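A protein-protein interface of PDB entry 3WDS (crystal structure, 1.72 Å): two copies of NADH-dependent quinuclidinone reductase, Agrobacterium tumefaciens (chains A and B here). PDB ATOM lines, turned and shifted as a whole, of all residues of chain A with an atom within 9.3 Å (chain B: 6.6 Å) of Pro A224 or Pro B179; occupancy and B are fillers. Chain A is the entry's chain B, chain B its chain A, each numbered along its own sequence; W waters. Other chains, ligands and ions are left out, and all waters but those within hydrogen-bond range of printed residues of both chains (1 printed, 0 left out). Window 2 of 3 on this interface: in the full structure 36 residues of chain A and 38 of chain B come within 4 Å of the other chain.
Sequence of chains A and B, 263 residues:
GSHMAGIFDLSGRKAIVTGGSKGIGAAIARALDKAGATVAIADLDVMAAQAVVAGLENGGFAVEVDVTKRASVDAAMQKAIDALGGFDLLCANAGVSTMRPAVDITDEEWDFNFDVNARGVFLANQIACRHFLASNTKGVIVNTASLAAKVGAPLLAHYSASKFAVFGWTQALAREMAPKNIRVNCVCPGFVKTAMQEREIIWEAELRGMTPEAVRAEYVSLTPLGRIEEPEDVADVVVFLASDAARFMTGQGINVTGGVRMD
Of the 10 printed residues of chain B, 5 touch a printed residue of chain A.
Hydrophobic or aromatic side chains of chain B that line the printed part of chain A: Ala B174, Ala B178 and Pro B179.
Among the printed residues, 10 pairs touch across the chains.
Among the printed residues, pairs that only touch across the chains: Pro A224 with Arg B175 (3.9 Å), Pro A224 with Ala B178 (3.3 Å), Pro A224 with Pro B179 (3.6 Å), Leu A225 with Ala B178 (3.7 Å), Gly A259 with Thr B250 (3.7 Å), Met A262 with Ala B174 (3.9 Å) and Met A262 with Thr B250 (3.6 Å).
Water W1 bridges N of Met A262 (2.9 Å) and NH2 of Arg B175 (3.2 Å).
No position is printed for both chains.
Of the 10 pairs that touch across the chains among the printed residues, none has its exchanged pair printed and touching as well.
Of the printed residues of chain B, Pro A224 touches Arg B175 (3.9 Å), Ala B178 (3.3 Å) and Pro B179 (3.6 Å).
Of chain A, only Pro A224 (3.6 Å) comes within 4 Å of Pro B179.
Of the printed residues of chain A, Thr B250 touches Gly A259 and Met A262.
Of the printed residues of chain A, Arg B175 touches Pro A224 (3.9 Å), Gly A259 (3.4 Å), Val A260 (3.4 Å) and Met A262 (3.7 Å).
Of the printed residues of chain A, Ala B174 touches Met A262.
Asn B181 touches none of the printed residues of chain A.
The nearest residue of chain B that does not touch Pro A224 is Thr B250 (4.9 Å).
The nearest residue of chain A that does not touch Pro B179 is Leu A225 (5.2 Å).
The backbone NH (N) of Gly A259 lies close to the side-chain hydroxyl (OG1) of Thr A257, 3.5 Å away.
The backbone NH of Leu A225 lies within hydrogen-bond range of the backbone carbonyl oxygen of Gly A258 (3.1 Å).
OG1 of Thr A257 lies within hydrogen-bond range of N of Val A260 (3.0 Å).
The guanidinium group (NH1) of Arg B175 is in hydrogen-bond range of the backbone carbonyl oxygen (O) of Gly A259 (3.4 Å).
NE of Arg B175 sits at hydrogen-bond distance from SD of Met A262, 3.7 Å away.
The guanidinium group (NH2) of Arg B175 sits at hydrogen-bond distance from the backbone carbonyl oxygen (O) of Val A260.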
ATOM      1  N   PHE A 191     -25.931  20.771  16.068  1.00  0.00           N
ATOM      2  CA  PHE A 191     -25.851  20.782  17.519  1.00  0.00           C
ATOM      3  C   PHE A 191     -27.254  20.926  18.063  1.00  0.00           C
ATOM      4  O   PHE A 191     -27.719  22.042  18.324  1.00  0.00           O
ATOM      5  CB  PHE A 191     -24.943  21.958  17.919  1.00  0.00           C
ATOM      6  CG  PHE A 191     -23.625  21.926  17.254  1.00  0.00           C
ATOM      7  CD1 PHE A 191     -22.897  20.783  17.263  1.00  0.00           C
ATOM      8  CD2 PHE A 191     -23.113  23.004  16.564  1.00  0.00           C
ATOM      9  CE1 PHE A 191     -21.664  20.680  16.612  1.00  0.00           C
ATOM     10  CE2 PHE A 191     -21.853  22.926  15.896  1.00  0.00           C
ATOM     11  CZ  PHE A 191     -21.115  21.756  15.969  1.00  0.00           C
ATOM     12  N   GLU A 218     -19.433  27.546  22.584  1.00  0.00           N
ATOM     13  CA  GLU A 218     -18.509  27.239  21.495  1.00  0.00           C
ATOM     14  C   GLU A 218     -19.324  26.669  20.330  1.00  0.00           C
ATOM     15  O   GLU A 218     -19.082  27.048  19.171  1.00  0.00           O
ATOM     16  CB  GLU A 218     -17.400  26.262  21.941  1.00  0.00           C
ATOM     17  CG  GLU A 218     -16.395  25.932  20.857  1.00  0.00           C
ATOM     18  CD  GLU A 218     -15.102  25.242  21.360  1.00  0.00           C
ATOM     19  OE1 GLU A 218     -14.980  24.893  22.540  1.00  0.00           O
ATOM     20  OE2 GLU A 218     -14.169  25.066  20.534  1.00  0.00           O
ATOM     21  N   TYR A 219     -20.294  25.814  20.635  1.00  0.00           N
ATOM     22  CA  TYR A 219     -21.185  25.208  19.580  1.00  0.00           C
ATOM     23  C   TYR A 219     -21.913  26.330  18.853  1.00  0.00           C
ATOM     24  O   TYR A 219     -21.914  26.338  17.637  1.00  0.00           O
ATOM     25  CB  TYR A 219     -22.198  24.249  20.171  1.00  0.00           C
ATOM     26  CG  TYR A 219     -21.532  22.951  20.517  1.00  0.00           C
ATOM     27  CD1 TYR A 219     -20.929  22.241  19.539  1.00  0.00           C
ATOM     28  CD2 TYR A 219     -21.413  22.505  21.800  1.00  0.00           C
ATOM     29  CE1 TYR A 219     -20.317  21.028  19.791  1.00  0.00           C
ATOM     30  CE2 TYR A 219     -20.811  21.283  22.070  1.00  0.00           C
ATOM     31  CZ  TYR A 219     -20.232  20.576  21.064  1.00  0.00           C
ATOM     32  OH  TYR A 219     -19.586  19.334  21.278  1.00  0.00           O
ATOM     33  N   VAL A 220     -22.442  27.309  19.606  1.00  0.00           N
ATOM     34  CA  VAL A 220     -23.169  28.390  18.972  1.00  0.00           C
ATOM     35  C   VAL A 220     -22.180  29.237  18.144  1.00  0.00           C
ATOM     36  O   VAL A 220     -22.495  29.614  17.019  1.00  0.00           O
ATOM     37  CB  VAL A 220     -23.917  29.273  19.956  1.00  0.00           C
ATOM     38  CG1 VAL A 220     -24.475  30.498  19.271  1.00  0.00           C
ATOM     39  CG2 VAL A 220     -25.004  28.450  20.645  1.00  0.00           C
ATOM     40  N   SER A 221     -20.986  29.496  18.670  1.00  0.00           N
ATOM     41  CA  SER A 221     -19.991  30.280  17.919  1.00  0.00           C
ATOM     42  C   SER A 221     -19.577  29.624  16.607  1.00  0.00           C
ATOM     43  O   SER A 221     -19.266  30.334  15.604  1.00  0.00           O
ATOM     44  CB  SER A 221     -18.720  30.527  18.741  1.00  0.00           C
ATOM     45  OG  SER A 221     -19.118  31.381  19.791  1.00  0.00           O
ATOM     46  N   LEU A 222     -19.591  28.300  16.572  1.00  0.00           N
ATOM     47  CA  LEU A 222     -19.311  27.544  15.357  1.00  0.00           C
ATOM     48  C   LEU A 222     -20.456  27.570  14.302  1.00  0.00           C
ATOM     49  O   LEU A 222     -20.286  27.097  13.204  1.00  0.00           O
ATOM     50  CB  LEU A 222     -18.993  26.105  15.715  1.00  0.00           C
ATOM     51  CG  LEU A 222     -17.633  25.848  16.418  1.00  0.00           C
ATOM     52  CD1 LEU A 222     -17.482  24.372  16.799  1.00  0.00           C
ATOM     53  CD2 LEU A 222     -16.454  26.228  15.525  1.00  0.00           C
ATOM     54  N   THR A 223     -21.633  28.054  14.673  1.00  0.00           N
ATOM     55  CA  THR A 223     -22.806  27.878  13.877  1.00  0.00           C
ATOM     56  C   THR A 223     -23.060  29.221  13.135  1.00  0.00           C
ATOM     57  O   THR A 223     -23.386  30.182  13.767  1.00  0.00           O
ATOM     58  CB  THR A 223     -24.024  27.580  14.783  1.00  0.00           C
ATOM     59  OG1 THR A 223     -23.738  26.356  15.528  1.00  0.00           O
ATOM     60  CG2 THR A 223     -25.214  27.282  13.851  1.00  0.00           C
ATOM     61  N   PRO A 224     -22.975  29.261  11.819  1.00  0.00           N
ATOM     62  CA  PRO A 224     -23.175  30.561  11.118  1.00  0.00           C
ATOM     63  C   PRO A 224     -24.527  31.194  11.393  1.00  0.00           C
ATOM     64  O   PRO A 224     -24.611  32.415  11.601  1.00  0.00           O
ATOM     65  CB  PRO A 224     -23.041  30.159   9.651  1.00  0.00           C
ATOM     66  CG  PRO A 224     -22.005  29.084   9.745  1.00  0.00           C
ATOM     67  CD  PRO A 224     -22.325  28.280  10.960  1.00  0.00           C
ATOM     68  N   LEU A 225     -25.581  30.384  11.499  1.00  0.00           N
ATOM     69  CA  LEU A 225     -26.875  30.933  11.836  1.00  0.00           C
ATOM     70  C   LEU A 225     -27.053  31.446  13.271  1.00  0.00           C
ATOM     71  O   LEU A 225     -28.059  32.068  13.611  1.00  0.00           O
ATOM     72  CB  LEU A 225     -28.000  29.992  11.360  1.00  0.00           C
ATOM     73  CG  LEU A 225     -28.285  29.971   9.851  1.00  0.00           C
ATOM     74  CD1 LEU A 225     -29.376  28.953   9.582  1.00  0.00           C
ATOM     75  CD2 LEU A 225     -28.748  31.297   9.285  1.00  0.00           C
ATOM     76  N   GLY A 226     -26.105  31.188  14.150  1.00  0.00           N
ATOM     77  CA  GLY A 226     -25.984  31.974  15.399  1.00  0.00           C
ATOM     78  C   GLY A 226     -26.799  31.448  16.530  1.00  0.00           C
ATOM     79  O   GLY A 226     -27.041  32.205  17.526  1.00  0.00           O
ATOM     80  N   ARG A 227     -27.312  30.219  16.436  1.00  0.00           N
ATOM     81  CA  ARG A 227     -28.098  29.660  17.551  1.00  0.00           C
ATOM     82  C   ARG A 227     -27.982  28.157  17.590  1.00  0.00           C
ATOM     83  O   ARG A 227     -27.654  27.511  16.587  1.00  0.00           O
ATOM     84  CB  ARG A 227     -29.596  29.981  17.373  1.00  0.00           C
ATOM     85  CG  ARG A 227     -30.258  29.487  16.111  1.00  0.00           C
ATOM     86  CD  ARG A 227     -31.765  29.678  16.151  1.00  0.00           C
ATOM     87  NE  ARG A 227     -32.490  29.242  14.973  1.00  0.00           N
ATOM     88  CZ  ARG A 227     -32.982  27.974  14.855  1.00  0.00           C
ATOM     89  NH1 ARG A 227     -32.746  27.004  15.763  1.00  0.00           N
ATOM     90  NH2 ARG A 227     -33.657  27.667  13.792  1.00  0.00           N
ATOM     91  N   ILE A 228     -28.253  27.616  18.771  1.00  0.00           N
ATOM     92  CA  ILE A 228     -28.369  26.200  18.946  1.00  0.00           C
ATOM     93  C   ILE A 228     -29.589  25.670  18.153  1.00  0.00           C
ATOM     94  O   ILE A 228     -30.592  26.409  17.894  1.00  0.00           O
ATOM     95  CB  ILE A 228     -28.479  25.877  20.452  1.00  0.00           C
ATOM     96  CG1 ILE A 228     -28.018  24.491  20.712  1.00  0.00           C
ATOM     97  CG2 ILE A 228     -29.866  26.078  20.943  1.00  0.00           C
ATOM     98  CD1 ILE A 228     -26.476  24.470  20.643  1.00  0.00           C
ATOM     99  N   THR A 257     -27.661  21.940   9.743  1.00  0.00           N
ATOM    100  CA  THR A 257     -26.678  22.271  10.759  1.00  0.00           C
ATOM    101  C   THR A 257     -26.527  23.795  10.954  1.00  0.00           C
ATOM    102  O   THR A 257     -25.708  24.238  11.755  1.00  0.00           O
ATOM    103  CB  THR A 257     -25.249  21.739  10.375  1.00  0.00           C
ATOM    104  OG1 THR A 257     -24.722  22.529   9.299  1.00  0.00           O
ATOM    105  CG2 THR A 257     -25.253  20.306   9.982  1.00  0.00           C
ATOM    106  N   GLY A 258     -27.301  24.596  10.278  1.00  0.00           N
ATOM    107  CA  GLY A 258     -27.170  26.036  10.430  1.00  0.00           C
ATOM    108  C   GLY A 258     -25.946  26.595   9.770  1.00  0.00           C
ATOM    109  O   GLY A 258     -25.450  27.630  10.176  1.00  0.00           O
ATOM    110  N   GLY A 259     -25.420  25.874   8.763  1.00  0.00           N
ATOM    111  CA  GLY A 259     -24.230  26.428   8.066  1.00  0.00           C
ATOM    112  C   GLY A 259     -22.897  25.875   8.594  1.00  0.00           C
ATOM    113  O   GLY A 259     -21.822  26.169   8.029  1.00  0.00           O
ATOM    114  N   VAL A 260     -22.910  24.961   9.564  1.00  0.00           N
ATOM    115  CA  VAL A 260     -21.683  24.371  10.069  1.00  0.00           C
ATOM    116  C   VAL A 260     -20.956  23.597   9.006  1.00  0.00           C
ATOM    117  O   VAL A 260     -19.729  23.697   8.911  1.00  0.00           O
ATOM    118  CB  VAL A 260     -21.918  23.507  11.293  1.00  0.00           C
ATOM    119  CG1 VAL A 260     -20.670  22.780  11.778  1.00  0.00           C
ATOM    120  CG2 VAL A 260     -22.436  24.341  12.443  1.00  0.00           C
ATOM    121  N   ARG A 261     -21.695  22.784   8.277  1.00  0.00           N
ATOM    122  CA  ARG A 261     -21.152  21.861   7.304  1.00  0.00           C
ATOM    123  C   ARG A 261     -21.901  22.102   5.995  1.00  0.00           C
ATOM    124  O   ARG A 261     -23.120  22.151   6.015  1.00  0.00           O
ATOM    125  CB  ARG A 261     -21.331  20.417   7.750  1.00  0.00           C
ATOM    126  CG  ARG A 261     -20.967  19.440   6.663  1.00  0.00           C
ATOM    127  CD  ARG A 261     -19.485  19.334   6.400  1.00  0.00           C
ATOM    128  NE  ARG A 261     -19.198  18.417   5.314  1.00  0.00           N
ATOM    129  CZ  ARG A 261     -17.944  18.074   5.002  1.00  0.00           C
ATOM    130  NH1 ARG A 261     -16.936  18.460   5.764  1.00  0.00           N
ATOM    131  NH2 ARG A 261     -17.747  17.180   4.092  1.00  0.00           N
ATOM    132  N   MET A 262     -21.169  22.331   4.886  1.00  0.00           N
ATOM    133  CA  MET A 262     -21.726  22.601   3.554  1.00  0.00           C
ATOM    134  C   MET A 262     -21.312  21.525   2.554  1.00  0.00           C
ATOM    135  O   MET A 262     -20.112  21.343   2.354  1.00  0.00           O
ATOM    136  CB  MET A 262     -21.289  23.985   3.097  1.00  0.00           C
ATOM    137  CG  MET A 262     -21.867  25.036   4.039  1.00  0.00           C
ATOM    138  SD  MET A 262     -21.246  26.667   3.650  1.00  0.00           S
ATOM    139  CE  MET A 262     -22.183  27.599   4.883  1.00  0.00           C
ATOM    140  N   ALA B 174     -23.003  32.480   1.961  1.00  0.00           N
ATOM    141  CA  ALA B 174     -23.825  31.974   3.041  1.00  0.00           C
ATOM    142  C   ALA B 174     -23.190  32.285   4.417  1.00  0.00           C
ATOM    143  O   ALA B 174     -23.851  32.601   5.380  1.00  0.00           O
ATOM    144  CB  ALA B 174     -24.054  30.462   2.908  1.00  0.00           C
ATOM    145  N   ARG B 175     -21.873  32.073   4.524  1.00  0.00           N
ATOM    146  CA  ARG B 175     -21.165  32.267   5.788  1.00  0.00           C
ATOM    147  C   ARG B 175     -21.222  33.751   6.181  1.00  0.00           C
ATOM    148  O   ARG B 175     -21.430  34.029   7.337  1.00  0.00           O
ATOM    149  CB  ARG B 175     -19.722  31.762   5.707  1.00  0.00           C
ATOM    150  CG  ARG B 175     -19.717  30.247   5.840  1.00  0.00           C
ATOM    151  CD  ARG B 175     -18.360  29.561   5.680  1.00  0.00           C
ATOM    152  NE  ARG B 175     -18.477  28.065   5.747  1.00  0.00           N
ATOM    153  CZ  ARG B 175     -18.639  27.245   6.831  1.00  0.00           C
ATOM    154  NH1 ARG B 175     -18.757  27.670   8.094  1.00  0.00           N
ATOM    155  NH2 ARG B 175     -18.655  25.926   6.622  1.00  0.00           N
ATOM    156  N   GLU B 176     -21.121  34.654   5.229  1.00  0.00           N
ATOM    157  CA  GLU B 176     -21.209  36.096   5.506  1.00  0.00           C
ATOM    158  C   GLU B 176     -22.599  36.529   5.841  1.00  0.00           C
ATOM    159  O   GLU B 176     -22.784  37.470   6.623  1.00  0.00           O
ATOM    160  CB  GLU B 176     -20.725  36.929   4.326  1.00  0.00           C
ATOM    161  CG  GLU B 176     -19.272  36.815   4.075  1.00  0.00           C
ATOM    162  CD  GLU B 176     -18.700  37.889   3.162  1.00  0.00           C
ATOM    163  OE1 GLU B 176     -19.014  39.117   3.287  1.00  0.00           O
ATOM    164  OE2 GLU B 176     -17.860  37.521   2.345  1.00  0.00           O
ATOM    165  N   MET B 177     -23.610  35.921   5.213  1.00  0.00           N
ATOM    166  CA  MET B 177     -24.932  36.399   5.403  1.00  0.00           C
ATOM    167  C   MET B 177     -25.661  35.726   6.554  1.00  0.00           C
ATOM    168  O   MET B 177     -26.659  36.216   6.948  1.00  0.00           O
ATOM    169  CB  MET B 177     -25.750  36.279   4.139  1.00  0.00           C
ATOM    170  CG  MET B 177     -25.201  37.051   2.992  1.00  0.00           C
ATOM    171  SD  MET B 177     -25.649  38.845   3.293  1.00  0.00           S
ATOM    172  CE  MET B 177     -23.969  39.368   3.261  1.00  0.00           C
ATOM    173  N   ALA B 178     -25.169  34.602   7.083  1.00  0.00           N
ATOM    174  CA  ALA B 178     -25.889  33.831   8.051  1.00  0.00           C
ATOM    175  C   ALA B 178     -26.147  34.652   9.356  1.00  0.00           C
ATOM    176  O   ALA B 178     -27.251  34.569   9.927  1.00  0.00           O
ATOM    177  CB  ALA B 178     -25.084  32.578   8.336  1.00  0.00           C
ATOM    178  N   PRO B 179     -25.161  35.430   9.771  1.00  0.00           N
ATOM    179  CA  PRO B 179     -25.411  36.270  10.969  1.00  0.00           C
ATOM    180  C   PRO B 179     -26.486  37.323  10.819  1.00  0.00           C
ATOM    181  O   PRO B 179     -26.912  37.910  11.856  1.00  0.00           O
ATOM    182  CB  PRO B 179     -24.080  36.973  11.204  1.00  0.00           C
ATOM    183  CG  PRO B 179     -23.075  36.152  10.459  1.00  0.00           C
ATOM    184  CD  PRO B 179     -23.766  35.530   9.319  1.00  0.00           C
ATOM    185  N   LYS B 180     -26.826  37.646   9.581  1.00  0.00           N
ATOM    186  CA  LYS B 180     -27.826  38.640   9.252  1.00  0.00           C
ATOM    187  C   LYS B 180     -29.151  37.980   8.793  1.00  0.00           C
ATOM    188  O   LYS B 180     -29.988  38.623   8.191  1.00  0.00           O
ATOM    189  CB  LYS B 180     -27.257  39.606   8.250  1.00  0.00           C
ATOM    190  CG  LYS B 180     -26.568  40.784   8.945  1.00  0.00           C
ATOM    191  CD  LYS B 180     -25.170  40.997   8.436  1.00  0.00           C
ATOM    192  CE  LYS B 180     -24.294  41.629   9.514  1.00  0.00           C
ATOM    193  NZ  LYS B 180     -24.616  43.074   9.675  1.00  0.00           N
ATOM    194  N   ASN B 181     -29.322  36.699   9.057  1.00  0.00           N
ATOM    195  CA  ASN B 181     -30.630  36.085   8.948  1.00  0.00           C
ATOM    196  C   ASN B 181     -30.984  35.846   7.457  1.00  0.00           C
ATOM    197  O   ASN B 181     -32.171  35.691   7.115  1.00  0.00           O
ATOM    198  CB  ASN B 181     -31.669  37.041   9.592  1.00  0.00           C
ATOM    199  CG  ASN B 181     -32.978  36.362   9.968  1.00  0.00           C
ATOM    200  OD1 ASN B 181     -33.005  35.168  10.292  1.00  0.00           O
ATOM    201  ND2 ASN B 181     -34.096  37.161   9.996  1.00  0.00           N
ATOM    202  N   ILE B 182     -29.981  35.827   6.578  1.00  0.00           N
ATOM    203  CA  ILE B 182     -30.223  35.633   5.169  1.00  0.00           C
ATOM    204  C   ILE B 182     -29.605  34.305   4.796  1.00  0.00           C
ATOM    205  O   ILE B 182     -28.437  34.114   5.047  1.00  0.00           O
ATOM    206  CB  ILE B 182     -29.526  36.737   4.367  1.00  0.00           C
ATOM    207  CG1 ILE B 182     -30.233  38.070   4.680  1.00  0.00           C
ATOM    208  CG2 ILE B 182     -29.443  36.397   2.907  1.00  0.00           C
ATOM    209  CD1 ILE B 182     -29.421  39.303   4.338  1.00  0.00           C
ATOM    210  N   THR B 250     -28.088  26.442   5.189  1.00  0.00           N
ATOM    211  CA  THR B 250     -27.508  27.503   4.371  1.00  0.00           C
ATOM    212  C   THR B 250     -26.155  27.062   3.917  1.00  0.00           C
ATOM    213  O   THR B 250     -25.521  26.253   4.589  1.00  0.00           O
ATOM    214  CB  THR B 250     -27.438  28.821   5.143  1.00  0.00           C
ATOM    215  OG1 THR B 250     -27.216  29.864   4.205  1.00  0.00           O
ATOM    216  CG2 THR B 250     -26.375  28.843   6.262  1.00  0.00           C
HETATM  217  O   HOH W   1     -18.376  22.986   5.311  1.00  0.00           O
